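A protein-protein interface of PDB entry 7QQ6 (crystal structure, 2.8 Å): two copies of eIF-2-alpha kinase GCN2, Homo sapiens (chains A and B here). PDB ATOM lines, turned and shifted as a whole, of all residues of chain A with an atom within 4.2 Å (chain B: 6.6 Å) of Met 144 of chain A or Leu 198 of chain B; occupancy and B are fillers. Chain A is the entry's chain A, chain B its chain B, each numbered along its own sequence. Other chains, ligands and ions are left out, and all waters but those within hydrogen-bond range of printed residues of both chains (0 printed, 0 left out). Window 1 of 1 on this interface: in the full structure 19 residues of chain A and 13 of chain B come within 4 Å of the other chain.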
ATOM      1  N   LEU A  65      -6.924  24.891 -10.362  1.00  0.00           N
ATOM      2  CA  LEU A  65      -8.335  24.590 -10.606  1.00  0.00           C
ATOM      3  C   LEU A  65      -9.273  25.137  -9.560  1.00  0.00           C
ATOM      4  O   LEU A  65     -10.340  25.629  -9.908  1.00  0.00           O
ATOM      5  CB  LEU A  65      -8.553  23.074 -10.792  1.00  0.00           C
ATOM      6  CG  LEU A  65      -7.926  22.424 -12.029  1.00  0.00           C
ATOM      7  CD1 LEU A  65      -8.168  20.935 -12.036  1.00  0.00           C
ATOM      8  CD2 LEU A  65      -8.444  23.036 -13.318  1.00  0.00           C
ATOM      9  N   LEU A  69     -12.571  28.214  -9.196  1.00  0.00           N
ATOM     10  CA  LEU A  69     -13.927  27.809  -8.828  1.00  0.00           C
ATOM     11  C   LEU A  69     -14.565  28.921  -7.998  1.00  0.00           C
ATOM     12  O   LEU A  69     -13.954  29.363  -7.027  1.00  0.00           O
ATOM     13  CB  LEU A  69     -13.919  26.471  -8.057  1.00  0.00           C
ATOM     14  CG  LEU A  69     -13.767  25.228  -8.916  1.00  0.00           C
ATOM     15  CD1 LEU A  69     -13.068  24.122  -8.154  1.00  0.00           C
ATOM     16  CD2 LEU A  69     -15.101  24.740  -9.409  1.00  0.00           C
ATOM     17  N   ILE A 139     -19.200  22.610 -10.624  1.00  0.00           N
ATOM     18  CA  ILE A 139     -17.907  21.921 -10.750  1.00  0.00           C
ATOM     19  C   ILE A 139     -17.894  21.183 -12.080  1.00  0.00           C
ATOM     20  O   ILE A 139     -16.946  21.327 -12.840  1.00  0.00           O
ATOM     21  CB  ILE A 139     -17.646  20.960  -9.539  1.00  0.00           C
ATOM     22  CG1 ILE A 139     -17.394  21.742  -8.233  1.00  0.00           C
ATOM     23  CG2 ILE A 139     -16.484  19.990  -9.813  1.00  0.00           C
ATOM     24  CD1 ILE A 139     -17.671  20.928  -6.897  1.00  0.00           C
ATOM     25  N   HIS A 140     -18.983  20.443 -12.362  1.00  0.00           N
ATOM     26  CA  HIS A 140     -19.210  19.599 -13.530  1.00  0.00           C
ATOM     27  C   HIS A 140     -19.348  20.340 -14.819  1.00  0.00           C
ATOM     28  O   HIS A 140     -18.900  19.813 -15.827  1.00  0.00           O
ATOM     29  CB  HIS A 140     -20.424  18.694 -13.309  1.00  0.00           C
ATOM     30  CG  HIS A 140     -20.133  17.498 -12.465  1.00  0.00           C
ATOM     31  ND1 HIS A 140     -21.054  16.485 -12.328  1.00  0.00           N
ATOM     32  CD2 HIS A 140     -19.019  17.180 -11.762  1.00  0.00           C
ATOM     33  CE1 HIS A 140     -20.480  15.586 -11.544  1.00  0.00           C
ATOM     34  NE2 HIS A 140     -19.251  15.965 -11.182  1.00  0.00           N
ATOM     35  N   LYS A 142     -17.873  23.147 -15.411  1.00  0.00           N
ATOM     36  CA  LYS A 142     -16.540  23.709 -15.596  1.00  0.00           C
ATOM     37  C   LYS A 142     -15.590  22.541 -15.915  1.00  0.00           C
ATOM     38  O   LYS A 142     -14.368  22.667 -15.785  1.00  0.00           O
ATOM     39  CB  LYS A 142     -16.096  24.501 -14.350  1.00  0.00           C
ATOM     40  CG  LYS A 142     -16.860  25.790 -14.182  1.00  0.00           C
ATOM     41  CD  LYS A 142     -15.975  26.874 -13.669  1.00  0.00           C
ATOM     42  CE  LYS A 142     -16.319  28.197 -14.306  1.00  0.00           C
ATOM     43  NZ  LYS A 142     -15.449  29.294 -13.795  1.00  0.00           N
ATOM     44  N   GLY A 143     -16.193  21.422 -16.349  1.00  0.00           N
ATOM     45  CA  GLY A 143     -15.551  20.176 -16.755  1.00  0.00           C
ATOM     46  C   GLY A 143     -14.506  19.705 -15.779  1.00  0.00           C
ATOM     47  O   GLY A 143     -13.318  19.912 -16.008  1.00  0.00           O
ATOM     48  N   MET A 144     -14.945  19.128 -14.657  1.00  0.00           N
ATOM     49  CA  MET A 144     -14.106  18.632 -13.577  1.00  0.00           C
ATOM     50  C   MET A 144     -14.836  17.512 -12.878  1.00  0.00           C
ATOM     51  O   MET A 144     -16.056  17.421 -12.934  1.00  0.00           O
ATOM     52  CB  MET A 144     -13.791  19.756 -12.557  1.00  0.00           C
ATOM     53  CG  MET A 144     -12.618  20.656 -12.962  1.00  0.00           C
ATOM     54  SD  MET A 144     -12.208  22.016 -11.837  1.00  0.00           S
ATOM     55  CE  MET A 144     -13.315  23.209 -12.338  1.00  0.00           C
ATOM     56  N   ILE A 145     -14.069  16.648 -12.228  1.00  0.00           N
ATOM     57  CA  ILE A 145     -14.513  15.540 -11.408  1.00  0.00           C
ATOM     58  C   ILE A 145     -13.924  15.856 -10.039  1.00  0.00           C
ATOM     59  O   ILE A 145     -12.763  16.259  -9.969  1.00  0.00           O
ATOM     60  CB  ILE A 145     -14.007  14.186 -11.970  1.00  0.00           C
ATOM     61  CG1 ILE A 145     -14.462  14.005 -13.439  1.00  0.00           C
ATOM     62  CG2 ILE A 145     -14.500  13.011 -11.084  1.00  0.00           C
ATOM     63  CD1 ILE A 145     -13.464  13.381 -14.351  1.00  0.00           C
ATOM     64  N   GLN A 222     -17.506  11.805 -14.547  1.00  0.00           N
ATOM     65  CA  GLN A 222     -18.215  12.765 -13.711  1.00  0.00           C
ATOM     66  C   GLN A 222     -19.369  12.037 -12.985  1.00  0.00           C
ATOM     67  O   GLN A 222     -19.825  12.489 -11.931  1.00  0.00           O
ATOM     68  CB  GLN A 222     -18.747  13.918 -14.562  1.00  0.00           C
ATOM     69  CG  GLN A 222     -17.661  14.876 -15.064  1.00  0.00           C
ATOM     70  CD  GLN A 222     -18.222  16.106 -15.721  1.00  0.00           C
ATOM     71  OE1 GLN A 222     -19.365  16.126 -16.187  1.00  0.00           O
ATOM     72  NE2 GLN A 222     -17.428  17.162 -15.776  1.00  0.00           N
ATOM     73  N   ASP B 188     -14.585  10.063 -18.622  1.00  0.00           N
ATOM     74  CA  ASP B 188     -14.226  11.242 -19.404  1.00  0.00           C
ATOM     75  C   ASP B 188     -13.035  12.010 -18.813  1.00  0.00           C
ATOM     76  O   ASP B 188     -12.759  13.124 -19.272  1.00  0.00           O
ATOM     77  CB  ASP B 188     -15.442  12.167 -19.666  1.00  0.00           C
ATOM     78  CG  ASP B 188     -16.275  12.565 -18.458  1.00  0.00           C
ATOM     79  OD1 ASP B 188     -15.713  12.647 -17.342  1.00  0.00           O
ATOM     80  OD2 ASP B 188     -17.491  12.814 -18.631  1.00  0.00           O
ATOM     81  N   LEU B 189     -12.311  11.419 -17.827  1.00  0.00           N
ATOM     82  CA  LEU B 189     -11.114  12.044 -17.240  1.00  0.00           C
ATOM     83  C   LEU B 189      -9.970  11.971 -18.254  1.00  0.00           C
ATOM     84  O   LEU B 189      -9.718  10.910 -18.843  1.00  0.00           O
ATOM     85  CB  LEU B 189     -10.715  11.397 -15.893  1.00  0.00           C
ATOM     86  CG  LEU B 189      -9.289  11.628 -15.362  1.00  0.00           C
ATOM     87  CD1 LEU B 189      -9.078  13.051 -14.898  1.00  0.00           C
ATOM     88  CD2 LEU B 189      -8.975  10.680 -14.243  1.00  0.00           C
ATOM     89  N   ILE B 190      -9.296  13.104 -18.473  1.00  0.00           N
ATOM     90  CA  ILE B 190      -8.204  13.140 -19.424  1.00  0.00           C
ATOM     91  C   ILE B 190      -6.888  12.810 -18.679  1.00  0.00           C
ATOM     92  O   ILE B 190      -6.417  13.577 -17.834  1.00  0.00           O
ATOM     93  CB  ILE B 190      -8.200  14.427 -20.309  1.00  0.00           C
ATOM     94  CG1 ILE B 190      -7.754  15.692 -19.582  1.00  0.00           C
ATOM     95  CG2 ILE B 190      -9.553  14.645 -20.960  1.00  0.00           C
ATOM     96  CD1 ILE B 190      -6.446  16.188 -20.084  1.00  0.00           C
ATOM     97  N   LYS B 191      -6.362  11.599 -18.959  1.00  0.00           N
ATOM     98  CA  LYS B 191      -5.148  10.998 -18.401  1.00  0.00           C
ATOM     99  C   LYS B 191      -3.886  11.899 -18.465  1.00  0.00           C
ATOM    100  O   LYS B 191      -2.971  11.726 -17.652  1.00  0.00           O
ATOM    101  CB  LYS B 191      -4.889   9.638 -19.083  1.00  0.00           C
ATOM    102  CG  LYS B 191      -4.312   8.564 -18.155  1.00  0.00           C
ATOM    103  CD  LYS B 191      -2.780   8.428 -18.265  1.00  0.00           C
ATOM    104  CE  LYS B 191      -2.136   7.831 -17.028  1.00  0.00           C
ATOM    105  NZ  LYS B 191      -2.184   8.753 -15.857  1.00  0.00           N
ATOM    106  N   ASP B 193      -3.772  15.119 -17.777  1.00  0.00           N
ATOM    107  CA  ASP B 193      -3.878  16.118 -16.702  1.00  0.00           C
ATOM    108  C   ASP B 193      -3.227  15.631 -15.394  1.00  0.00           C
ATOM    109  O   ASP B 193      -3.631  14.578 -14.877  1.00  0.00           O
ATOM    110  CB  ASP B 193      -5.355  16.528 -16.492  1.00  0.00           C
ATOM    111  CG  ASP B 193      -5.667  17.360 -15.256  1.00  0.00           C
ATOM    112  OD1 ASP B 193      -4.954  18.363 -15.013  1.00  0.00           O
ATOM    113  OD2 ASP B 193      -6.638  17.018 -14.541  1.00  0.00           O
ATOM    114  N   SER B 195      -3.389  16.928 -12.225  1.00  0.00           N
ATOM    115  CA  SER B 195      -4.296  17.054 -11.069  1.00  0.00           C
ATOM    116  C   SER B 195      -5.182  15.814 -10.905  1.00  0.00           C
ATOM    117  O   SER B 195      -5.342  15.326  -9.786  1.00  0.00           O
ATOM    118  CB  SER B 195      -5.149  18.319 -11.174  1.00  0.00           C
ATOM    119  OG  SER B 195      -6.123  18.266 -12.207  1.00  0.00           O
ATOM    120  N   GLY B 196      -5.712  15.314 -12.024  1.00  0.00           N
ATOM    121  CA  GLY B 196      -6.567  14.136 -12.086  1.00  0.00           C
ATOM    122  C   GLY B 196      -8.039  14.448 -11.932  1.00  0.00           C
ATOM    123  O   GLY B 196      -8.816  13.585 -11.516  1.00  0.00           O
ATOM    124  N   HIS B 197      -8.446  15.668 -12.315  1.00  0.00           N
ATOM    125  CA  HIS B 197      -9.834  16.120 -12.193  1.00  0.00           C
ATOM    126  C   HIS B 197     -10.464  16.561 -13.516  1.00  0.00           C
ATOM    127  O   HIS B 197     -11.659  16.352 -13.703  1.00  0.00           O
ATOM    128  CB  HIS B 197      -9.944  17.241 -11.139  1.00  0.00           C
ATOM    129  CG  HIS B 197      -9.421  16.845  -9.791  1.00  0.00           C
ATOM    130  ND1 HIS B 197     -10.160  16.044  -8.934  1.00  0.00           N
ATOM    131  CD2 HIS B 197      -8.234  17.127  -9.208  1.00  0.00           C
ATOM    132  CE1 HIS B 197      -9.399  15.865  -7.867  1.00  0.00           C
ATOM    133  NE2 HIS B 197      -8.232  16.500  -7.986  1.00  0.00           N
ATOM    134  N   LEU B 198      -9.665  17.141 -14.433  1.00  0.00           N
ATOM    135  CA  LEU B 198     -10.135  17.701 -15.713  1.00  0.00           C
ATOM    136  C   LEU B 198     -10.686  16.689 -16.726  1.00  0.00           C
ATOM    137  O   LEU B 198     -10.166  15.588 -16.881  1.00  0.00           O
ATOM    138  CB  LEU B 198      -9.081  18.587 -16.371  1.00  0.00           C
ATOM    139  CG  LEU B 198      -8.895  19.952 -15.711  1.00  0.00           C
ATOM    140  CD1 LEU B 198      -7.616  20.578 -16.149  1.00  0.00           C
ATOM    141  CD2 LEU B 198     -10.077  20.874 -15.988  1.00  0.00           C
ATOM    142  N   THR B 199     -11.757  17.129 -17.413  1.00  0.00           N
ATOM    143  CA  THR B 199     -12.608  16.456 -18.394  1.00  0.00           C
ATOM    144  C   THR B 199     -12.645  17.281 -19.690  1.00  0.00           C
ATOM    145  O   THR B 199     -12.620  18.517 -19.639  1.00  0.00           O
ATOM    146  CB  THR B 199     -14.017  16.330 -17.750  1.00  0.00           C
ATOM    147  OG1 THR B 199     -14.112  15.074 -17.089  1.00  0.00           O
ATOM    148  CG2 THR B 199     -15.189  16.505 -18.731  1.00  0.00           C
ATOM    149  N   GLY B 200     -12.726  16.592 -20.825  1.00  0.00           N
ATOM    150  CA  GLY B 200     -12.856  17.250 -22.116  1.00  0.00           C
ATOM    151  C   GLY B 200     -11.765  17.032 -23.141  1.00  0.00           C
ATOM    152  O   GLY B 200     -11.134  15.971 -23.195  1.00  0.00           O
ATOM    153  N   ALA B 244      -0.315  22.169 -17.414  1.00  0.00           N
ATOM    154  CA  ALA B 244      -1.140  21.344 -18.288  1.00  0.00           C
ATOM    155  C   ALA B 244      -2.569  21.558 -17.825  1.00  0.00           C
ATOM    156  O   ALA B 244      -3.415  21.909 -18.640  1.00  0.00           O
ATOM    157  CB  ALA B 244      -0.756  19.885 -18.141  1.00  0.00           C
ATOM    158  N   SER B 245      -2.808  21.451 -16.488  1.00  0.00           N
ATOM    159  CA  SER B 245      -4.094  21.696 -15.820  1.00  0.00           C
ATOM    160  C   SER B 245      -4.690  23.081 -16.220  1.00  0.00           C
ATOM    161  O   SER B 245      -5.892  23.155 -16.484  1.00  0.00           O
ATOM    162  CB  SER B 245      -3.951  21.585 -14.300  1.00  0.00           C
ATOM    163  OG  SER B 245      -3.317  20.383 -13.889  1.00  0.00           O
ATOM    164  N   GLU B 246      -3.850  24.155 -16.317  1.00  0.00           N
ATOM    165  CA  GLU B 246      -4.336  25.471 -16.734  1.00  0.00           C
ATOM    166  C   GLU B 246      -4.756  25.456 -18.199  1.00  0.00           C
ATOM    167  O   GLU B 246      -5.909  25.777 -18.475  1.00  0.00           O
ATOM    168  CB  GLU B 246      -3.334  26.599 -16.468  1.00  0.00           C
ATOM    169  CG  GLU B 246      -3.982  27.960 -16.677  1.00  0.00           C
ATOM    170  CD  GLU B 246      -3.115  29.193 -16.552  1.00  0.00           C
ATOM    171  OE1 GLU B 246      -1.989  29.084 -16.015  1.00  0.00           O
ATOM    172  OE2 GLU B 246      -3.573  30.278 -16.980  1.00  0.00           O
ATOM    173  N   ARG B 247      -3.849  25.065 -19.131  1.00  0.00           N
ATOM    174  CA  ARG B 247      -4.163  25.001 -20.563  1.00  0.00           C
ATOM    175  C   ARG B 247      -5.429  24.181 -20.889  1.00  0.00           C
ATOM    176  O   ARG B 247      -6.240  24.640 -21.699  1.00  0.00           O
ATOM    177  CB  ARG B 247      -2.965  24.515 -21.399  1.00  0.00           C
ATOM    178  CG  ARG B 247      -2.892  25.225 -22.756  1.00  0.00           C
ATOM    179  CD  ARG B 247      -1.812  24.693 -23.669  1.00  0.00           C
ATOM    180  NE  ARG B 247      -2.348  23.678 -24.573  1.00  0.00           N
ATOM    181  CZ  ARG B 247      -2.808  23.937 -25.791  1.00  0.00           C
ATOM    182  NH1 ARG B 247      -2.791  25.175 -26.263  1.00  0.00           N
ATOM    183  NH2 ARG B 247      -3.282  22.955 -26.550  1.00  0.00           N
ATOM    184  N   ILE B 248      -5.610  22.989 -20.252  1.00  0.00           N
ATOM    185  CA  ILE B 248      -6.781  22.122 -20.490  1.00  0.00           C
ATOM    186  C   ILE B 248      -8.085  22.801 -20.042  1.00  0.00           C
ATOM    187  O   ILE B 248      -9.072  22.726 -20.767  1.00  0.00           O
ATOM    188  CB  ILE B 248      -6.664  20.668 -19.915  1.00  0.00           C
ATOM    189  CG1 ILE B 248      -5.239  20.053 -20.031  1.00  0.00           C
ATOM    190  CG2 ILE B 248      -7.725  19.723 -20.529  1.00  0.00           C
ATOM    191  CD1 ILE B 248      -4.656  19.856 -21.404  1.00  0.00           C
ATOM    192  N   PHE B 249      -8.082  23.453 -18.859  1.00  0.00           N
ATOM    193  CA  PHE B 249      -9.244  24.124 -18.269  1.00  0.00           C
ATOM    194  C   PHE B 249      -9.639  25.344 -19.058  1.00  0.00           C
ATOM    195  O   PHE B 249     -10.788  25.438 -19.488  1.00  0.00           O
ATOM    196  CB  PHE B 249      -8.987  24.492 -16.783  1.00  0.00           C
ATOM    197  CG  PHE B 249     -10.076  25.325 -16.133  1.00  0.00           C
ATOM    198  CD1 PHE B 249     -11.297  24.755 -15.784  1.00  0.00           C
ATOM    199  CD2 PHE B 249      -9.887  26.679 -15.893  1.00  0.00           C
ATOM    200  CE1 PHE B 249     -12.312  25.530 -15.226  1.00  0.00           C
ATOM    201  CE2 PHE B 249     -10.908  27.452 -15.345  1.00  0.00           C
ATOM    202  CZ  PHE B 249     -12.106  26.871 -15.004  1.00  0.00           C
ATOM    203  N   VAL B 250      -8.689  26.281 -19.225  1.00  0.00           N
ATOM    204  CA  VAL B 250      -8.825  27.554 -19.935  1.00  0.00           C
ATOM    205  C   VAL B 250      -9.293  27.369 -21.383  1.00  0.00           C
ATOM    206  O   VAL B 250     -10.220  28.071 -21.797  1.00  0.00           O
ATOM    207  CB  VAL B 250      -7.523  28.394 -19.840  1.00  0.00           C
ATOM    208  CG1 VAL B 250      -7.642  29.694 -20.618  1.00  0.00           C
ATOM    209  CG2 VAL B 250      -7.167  28.689 -18.390  1.00  0.00           C
ATOM    210  N   ASN B 252     -10.774  24.615 -22.735  1.00  0.00           N
ATOM    211  CA  ASN B 252     -12.054  23.881 -22.827  1.00  0.00           C
ATOM    212  C   ASN B 252     -13.239  24.754 -22.453  1.00  0.00           C
ATOM    213  O   ASN B 252     -14.375  24.464 -22.842  1.00  0.00           O
ATOM    214  CB  ASN B 252     -12.049  22.639 -21.962  1.00  0.00           C
ATOM    215  CG  ASN B 252     -11.650  21.405 -22.707  1.00  0.00           C
ATOM    216  OD1 ASN B 252     -12.452  20.807 -23.444  1.00  0.00           O
ATOM    217  ND2 ASN B 252     -10.407  20.986 -22.513  1.00  0.00           N
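Of the 19 printed residues of chain B, 7 touch a printed residue of chain A. Printed residues of chain B that touch a printed residue of chain A: Asp 188, Leu 189, Ser 195, His 197, Leu 198, Thr 199 and Phe 249. Among the printed residues, 15 pairs touch across the chains. Among the printed residues, no Asp or Glu carboxylate lies within 4 Å of a Lys or Arg side-chain nitrogen of the other chain.
OG of Ser 195 of chain B touches CD1 of Leu 65 of chain A, at 3.4 Å. Leu 198 of chain B touches Leu 65 of chain A (CD2 to CD2, 3.8 Å). CD2 of Leu 65 of chain A touches CB of Phe 249 of chain B, at 3.8 Å. O of Lys 142 of chain A touches CE1 of Phe 249 of chain B, 3.6 Å away. Leu 198 of chain B touches Gly 143 of chain A. Met 144 of chain A touches His 197 of chain B. CG of Met 144 of chain A touches CD2 of Leu 198 of chain B, 3.96 Å away. Met 144 of chain A touches Phe 249 of chain B. Ile 145 of chain A touches Asp 188 of chain B (CD1 to OD1, 3.8 Å). Ile 145 of chain A touches Thr 199 of chain B (CD1 to OG1, 3.3 Å).
O of Gly 143 of chain A is in hydrogen-bond range of N of Thr 199 of chain B, at 3.5 Å. O of Ile 145 of chain A lies within hydrogen-bond range of ND1 of His 197 of chain B, at 2.8 Å. N of Gln 222 of chain A lies within hydrogen-bond range of OD1 of Asp 188 of chain B (3.4 Å).
No position is printed for both chains. Of the 15 pairs that touch across the chains among the printed residues, none has its exchanged pair printed and touching as well.
Of the printed residues of chain B, Leu 65 of chain A touches Ser 195 (3.4 Å), Leu 198 (3.8 Å) and Phe 249 (3.8 Å). Met 144 of chain A touches just these residues of chain B: His 197, Leu 198 and Phe 249. Printed residues of chain A within 4 Å of Asp 188 of chain B: Ile 145 (3.8 Å) and Gln 222 (3.4 Å). Asp 193 of chain B touches none of the printed residues of chain A. Of the printed residues of chain A, Ser 195 of chain B touches Leu 65 (3.4 Å). Of the printed residues of chain A, His 197 of chain B touches Met 144 and Ile 145. Of the printed residues of chain A, Thr 199 of chain B touches Gly 143, Ile 145 and Gln 222. Val 250 of chain B touches none of the printed residues of chain A. The nearest residue of chain B that does not touch Met 144 of chain A is Thr 199 of chain B (4.3 Å). The nearest printed residue of chain A that does not touch Leu 198 of chain B is Lys 142 of chain A (4.7 Å). The nearest printed residue of chain B that does not touch Gln 222 of chain A is Leu 189 of chain B (6.2 Å).
The backbone carbonyl oxygen of Ile 139 of chain A lies within hydrogen-bond range of the backbone NH of Met 144 of chain A. The side-chain amide nitrogen (NE2) of Gln 222 of chain A lies within hydrogen-bond range of the backbone carbonyl oxygen (O) of His 140 of chain A (3.0 Å). NE2 of Gln 222 of chain A lies within hydrogen-bond range of O of Met 144 of chain A, at 3.2 Å. OD2 of Asp 193 of chain B is in hydrogen-bond range of OG of Ser 195 of chain B (2.7 Å). The backbone NH of His 197 of chain B lies within hydrogen-bond range of the side-chain carboxylate of Asp 193 of chain B, 3.2 Å away. The side-chain hydroxyl of Ser 195 of chain B sits at hydrogen-bond distance from the backbone NH of His 197 of chain B (3.5 Å).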
